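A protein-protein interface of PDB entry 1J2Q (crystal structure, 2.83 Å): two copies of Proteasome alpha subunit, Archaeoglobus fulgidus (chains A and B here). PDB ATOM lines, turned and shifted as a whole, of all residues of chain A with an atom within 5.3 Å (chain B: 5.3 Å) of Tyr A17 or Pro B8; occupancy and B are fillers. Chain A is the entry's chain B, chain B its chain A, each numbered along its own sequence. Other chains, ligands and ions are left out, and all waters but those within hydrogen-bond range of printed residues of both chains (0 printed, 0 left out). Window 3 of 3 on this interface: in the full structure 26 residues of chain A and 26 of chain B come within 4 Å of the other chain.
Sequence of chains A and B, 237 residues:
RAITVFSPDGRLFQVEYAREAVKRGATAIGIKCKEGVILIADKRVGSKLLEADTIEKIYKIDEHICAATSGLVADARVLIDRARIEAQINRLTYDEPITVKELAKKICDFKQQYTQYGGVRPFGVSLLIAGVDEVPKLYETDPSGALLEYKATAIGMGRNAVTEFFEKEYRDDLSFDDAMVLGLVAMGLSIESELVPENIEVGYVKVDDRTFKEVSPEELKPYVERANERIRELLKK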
ATOM      1  N   LEU A  12      13.249  -1.966 -14.448  1.00  0.00           N
ATOM      2  CA  LEU A  12      12.526  -1.846 -13.183  1.00  0.00           C
ATOM      3  C   LEU A  12      11.125  -2.411 -13.357  1.00  0.00           C
ATOM      4  O   LEU A  12      10.243  -1.756 -13.916  1.00  0.00           O
ATOM      5  CB  LEU A  12      12.435  -0.376 -12.776  1.00  0.00           C
ATOM      6  CG  LEU A  12      13.607   0.257 -12.032  1.00  0.00           C
ATOM      7  CD1 LEU A  12      14.873  -0.537 -12.239  1.00  0.00           C
ATOM      8  CD2 LEU A  12      13.763   1.698 -12.505  1.00  0.00           C
ATOM      9  N   PHE A  13      10.918  -3.626 -12.868  1.00  0.00           N
ATOM     10  CA  PHE A  13       9.627  -4.261 -13.024  1.00  0.00           C
ATOM     11  C   PHE A  13       8.463  -3.458 -12.469  1.00  0.00           C
ATOM     12  O   PHE A  13       7.409  -3.370 -13.110  1.00  0.00           O
ATOM     13  CB  PHE A  13       9.644  -5.680 -12.432  1.00  0.00           C
ATOM     14  CG  PHE A  13      10.323  -6.704 -13.318  1.00  0.00           C
ATOM     15  CD1 PHE A  13      10.255  -6.594 -14.722  1.00  0.00           C
ATOM     16  CD2 PHE A  13      11.039  -7.773 -12.761  1.00  0.00           C
ATOM     17  CE1 PHE A  13      10.883  -7.535 -15.562  1.00  0.00           C
ATOM     18  CE2 PHE A  13      11.672  -8.724 -13.586  1.00  0.00           C
ATOM     19  CZ  PHE A  13      11.597  -8.598 -14.991  1.00  0.00           C
ATOM     20  N   GLN A  14       8.628  -2.863 -11.294  1.00  0.00           N
ATOM     21  CA  GLN A  14       7.534  -2.082 -10.730  1.00  0.00           C
ATOM     22  C   GLN A  14       7.106  -0.998 -11.703  1.00  0.00           C
ATOM     23  O   GLN A  14       5.916  -0.756 -11.882  1.00  0.00           O
ATOM     24  CB  GLN A  14       7.937  -1.427  -9.410  1.00  0.00           C
ATOM     25  CG  GLN A  14       7.839  -2.316  -8.201  1.00  0.00           C
ATOM     26  CD  GLN A  14       6.491  -2.992  -8.087  1.00  0.00           C
ATOM     27  OE1 GLN A  14       6.273  -4.058  -8.667  1.00  0.00           O
ATOM     28  NE2 GLN A  14       5.571  -2.372  -7.347  1.00  0.00           N
ATOM     29  N   VAL A  15       8.086  -0.351 -12.330  1.00  0.00           N
ATOM     30  CA  VAL A  15       7.808   0.719 -13.279  1.00  0.00           C
ATOM     31  C   VAL A  15       7.096   0.165 -14.485  1.00  0.00           C
ATOM     32  O   VAL A  15       6.154   0.761 -14.986  1.00  0.00           O
ATOM     33  CB  VAL A  15       9.103   1.412 -13.755  1.00  0.00           C
ATOM     34  CG1 VAL A  15       8.778   2.449 -14.819  1.00  0.00           C
ATOM     35  CG2 VAL A  15       9.803   2.066 -12.585  1.00  0.00           C
ATOM     36  N   GLU A  16       7.552  -0.987 -14.952  1.00  0.00           N
ATOM     37  CA  GLU A  16       6.935  -1.601 -16.112  1.00  0.00           C
ATOM     38  C   GLU A  16       5.548  -2.101 -15.775  1.00  0.00           C
ATOM     39  O   GLU A  16       4.641  -2.011 -16.597  1.00  0.00           O
ATOM     40  CB  GLU A  16       7.816  -2.721 -16.645  1.00  0.00           C
ATOM     41  CG  GLU A  16       9.100  -2.180 -17.253  1.00  0.00           C
ATOM     42  CD  GLU A  16       9.950  -3.262 -17.895  1.00  0.00           C
ATOM     43  OE1 GLU A  16      11.072  -2.949 -18.364  1.00  0.00           O
ATOM     44  OE2 GLU A  16       9.493  -4.432 -17.929  1.00  0.00           O
ATOM     45  N   TYR A  17       5.372  -2.608 -14.567  1.00  0.00           N
ATOM     46  CA  TYR A  17       4.058  -3.069 -14.176  1.00  0.00           C
ATOM     47  C   TYR A  17       3.117  -1.872 -14.090  1.00  0.00           C
ATOM     48  O   TYR A  17       1.940  -1.970 -14.430  1.00  0.00           O
ATOM     49  CB  TYR A  17       4.114  -3.785 -12.826  1.00  0.00           C
ATOM     50  CG  TYR A  17       4.865  -5.086 -12.859  1.00  0.00           C
ATOM     51  CD1 TYR A  17       5.028  -5.791 -14.051  1.00  0.00           C
ATOM     52  CD2 TYR A  17       5.390  -5.633 -11.692  1.00  0.00           C
ATOM     53  CE1 TYR A  17       5.699  -7.014 -14.078  1.00  0.00           C
ATOM     54  CE2 TYR A  17       6.062  -6.851 -11.706  1.00  0.00           C
ATOM     55  CZ  TYR A  17       6.214  -7.537 -12.899  1.00  0.00           C
ATOM     56  OH  TYR A  17       6.871  -8.744 -12.918  1.00  0.00           O
ATOM     57  N   ALA A  18       3.643  -0.745 -13.625  1.00  0.00           N
ATOM     58  CA  ALA A  18       2.840   0.461 -13.515  1.00  0.00           C
ATOM     59  C   ALA A  18       2.362   0.809 -14.921  1.00  0.00           C
ATOM     60  O   ALA A  18       1.195   1.168 -15.131  1.00  0.00           O
ATOM     61  CB  ALA A  18       3.671   1.607 -12.931  1.00  0.00           C
ATOM     62  N   ARG A  19       3.267   0.684 -15.885  1.00  0.00           N
ATOM     63  CA  ARG A  19       2.927   0.970 -17.263  1.00  0.00           C
ATOM     64  C   ARG A  19       1.762   0.109 -17.729  1.00  0.00           C
ATOM     65  O   ARG A  19       0.910   0.564 -18.485  1.00  0.00           O
ATOM     66  CB  ARG A  19       4.148   0.786 -18.153  1.00  0.00           C
ATOM     67  CG  ARG A  19       5.077   1.988 -18.082  1.00  0.00           C
ATOM     68  CD  ARG A  19       6.011   2.085 -19.262  1.00  0.00           C
ATOM     69  NE  ARG A  19       7.220   1.282 -19.089  1.00  0.00           N
ATOM     70  CZ  ARG A  19       8.414   1.789 -18.786  1.00  0.00           C
ATOM     71  NH1 ARG A  19       8.569   3.099 -18.613  1.00  0.00           N
ATOM     72  NH2 ARG A  19       9.462   0.983 -18.680  1.00  0.00           N
ATOM     73  N   GLU A  20       1.711  -1.137 -17.270  1.00  0.00           N
ATOM     74  CA  GLU A  20       0.601  -2.013 -17.633  1.00  0.00           C
ATOM     75  C   GLU A  20      -0.716  -1.399 -17.180  1.00  0.00           C
ATOM     76  O   GLU A  20      -1.754  -1.602 -17.806  1.00  0.00           O
ATOM     77  CB  GLU A  20       0.757  -3.388 -16.990  1.00  0.00           C
ATOM     78  CG  GLU A  20       1.771  -4.238 -17.688  1.00  0.00           C
ATOM     79  CD  GLU A  20       1.568  -4.232 -19.192  1.00  0.00           C
ATOM     80  OE1 GLU A  20       0.444  -4.569 -19.646  1.00  0.00           O
ATOM     81  OE2 GLU A  20       2.532  -3.886 -19.917  1.00  0.00           O
ATOM     82  N   ALA A  21      -0.666  -0.649 -16.084  1.00  0.00           N
ATOM     83  CA  ALA A  21      -1.852  -0.006 -15.558  1.00  0.00           C
ATOM     84  C   ALA A  21      -2.323   1.113 -16.495  1.00  0.00           C
ATOM     85  O   ALA A  21      -3.523   1.241 -16.763  1.00  0.00           O
ATOM     86  CB  ALA A  21      -1.565   0.548 -14.172  1.00  0.00           C
ATOM     87  N   PHE B   6       2.613  -3.078  -7.274  1.00  0.00           N
ATOM     88  CA  PHE B   6       2.041  -3.462  -8.552  1.00  0.00           C
ATOM     89  C   PHE B   6       2.258  -4.929  -8.907  1.00  0.00           C
ATOM     90  O   PHE B   6       3.315  -5.510  -8.645  1.00  0.00           O
ATOM     91  CB  PHE B   6       2.626  -2.591  -9.667  1.00  0.00           C
ATOM     92  CG  PHE B   6       2.098  -1.188  -9.683  1.00  0.00           C
ATOM     93  CD1 PHE B   6       0.811  -0.925 -10.124  1.00  0.00           C
ATOM     94  CD2 PHE B   6       2.887  -0.129  -9.257  1.00  0.00           C
ATOM     95  CE1 PHE B   6       0.321   0.378 -10.141  1.00  0.00           C
ATOM     96  CE2 PHE B   6       2.404   1.169  -9.273  1.00  0.00           C
ATOM     97  CZ  PHE B   6       1.124   1.423  -9.713  1.00  0.00           C
ATOM     98  N   SER B   7       1.239  -5.528  -9.507  1.00  0.00           N
ATOM     99  CA  SER B   7       1.335  -6.911  -9.949  1.00  0.00           C
ATOM    100  C   SER B   7       1.735  -6.807 -11.413  1.00  0.00           C
ATOM    101  O   SER B   7       1.716  -5.720 -11.997  1.00  0.00           O
ATOM    102  CB  SER B   7      -0.022  -7.601  -9.870  1.00  0.00           C
ATOM    103  OG  SER B   7      -0.914  -7.062 -10.842  1.00  0.00           O
ATOM    104  N   PRO B   8       2.105  -7.928 -12.029  1.00  0.00           N
ATOM    105  CA  PRO B   8       2.484  -7.842 -13.441  1.00  0.00           C
ATOM    106  C   PRO B   8       1.320  -7.360 -14.319  1.00  0.00           C
ATOM    107  O   PRO B   8       1.522  -6.896 -15.441  1.00  0.00           O
ATOM    108  CB  PRO B   8       2.916  -9.266 -13.755  1.00  0.00           C
ATOM    109  CG  PRO B   8       3.511  -9.713 -12.440  1.00  0.00           C
ATOM    110  CD  PRO B   8       2.482  -9.230 -11.456  1.00  0.00           C
ATOM    111  N   ASP B   9       0.105  -7.462 -13.793  1.00  0.00           N
ATOM    112  CA  ASP B   9      -1.087  -7.028 -14.515  1.00  0.00           C
ATOM    113  C   ASP B   9      -1.250  -5.519 -14.413  1.00  0.00           C
ATOM    114  O   ASP B   9      -2.069  -4.930 -15.112  1.00  0.00           O
ATOM    115  CB  ASP B   9      -2.330  -7.691 -13.920  1.00  0.00           C
ATOM    116  CG  ASP B   9      -2.242  -9.212 -13.918  1.00  0.00           C
ATOM    117  OD1 ASP B   9      -2.938  -9.850 -13.085  1.00  0.00           O
ATOM    118  OD2 ASP B   9      -1.487  -9.764 -14.755  1.00  0.00           O
ATOM    119  N   GLY B  10      -0.475  -4.901 -13.528  1.00  0.00           N
ATOM    120  CA  GLY B  10      -0.561  -3.466 -13.347  1.00  0.00           C
ATOM    121  C   GLY B  10      -1.624  -3.122 -12.330  1.00  0.00           C
ATOM    122  O   GLY B  10      -2.150  -2.010 -12.309  1.00  0.00           O
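The backbone NH (N) of Phe B6 sits close to the side-chain amide nitrogen (NE2) of Gln A14, at 3.0 Å.
The side-chain hydroxyl (OG) of Ser B7 sits close to the backbone NH (N) of Asp B9 (3.1 Å).
N of Gly B10 is in hydrogen-bond range of OG of Ser B7 (3.5 Å).
CD2 of Tyr A17 touches O of Phe B6, at 3.7 Å.
CB of Tyr A17 touches O of Ser B7, 3.2 Å away.
CA of Pro B8 touches CD1 of Tyr A17, at 3.3 Å.
O of Tyr A17 touches CA of Gly B10, at 3.1 Å.
Ala A18 touches Phe B6 (CB to CE2, 3.9 Å).
Glu A20 touches Pro B8.
Glu A20 touches Asp B9.
Glu A20 touches Gly B10.
Ala A21 touches Gly B10 (CB to O, 3.2 Å).
Printed residues of chain B within 4 Å of Gln A14: Phe B6.
Of chain B, only Phe B6, Ser B7, Pro B8 and Gly B10 come within 4 Å of Tyr A17.
Printed residues of chain B within 4 Å of Glu A20: Pro B8, Asp B9 and Gly B10.
Pro B8 touches just these residues of chain A: Tyr A17 and Glu A20.
The nearest residue of chain B that does not touch Tyr A17 is Asp B9 (4.8 Å).
Of the 10 printed residues of chain A, 5 touch a printed residue of chain B.
Printed residues of chain A that touch a printed residue of chain B: Gln A14, Tyr A17, Ala A18, Glu A20 and Ala A21.
Hydrophobic or aromatic side chains of chain A that line the printed part of chain B: Tyr A17, Ala A18 and Ala A21.
Along chain A the printed residues that touch a printed residue of chain B span positions 14 to 21.
Printed residues of chain B that touch a printed residue of chain A: Phe B6, Ser B7, Pro B8, Asp B9 and Gly B10.
Hydrophobic or aromatic side chains of chain B within 4 Å of the printed part of chain A: Phe B6 and Pro B8.
No position is printed for both chains.
Of the 10 pairs that touch across the chains among the printed residues, none has its exchanged pair printed and touching as well.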
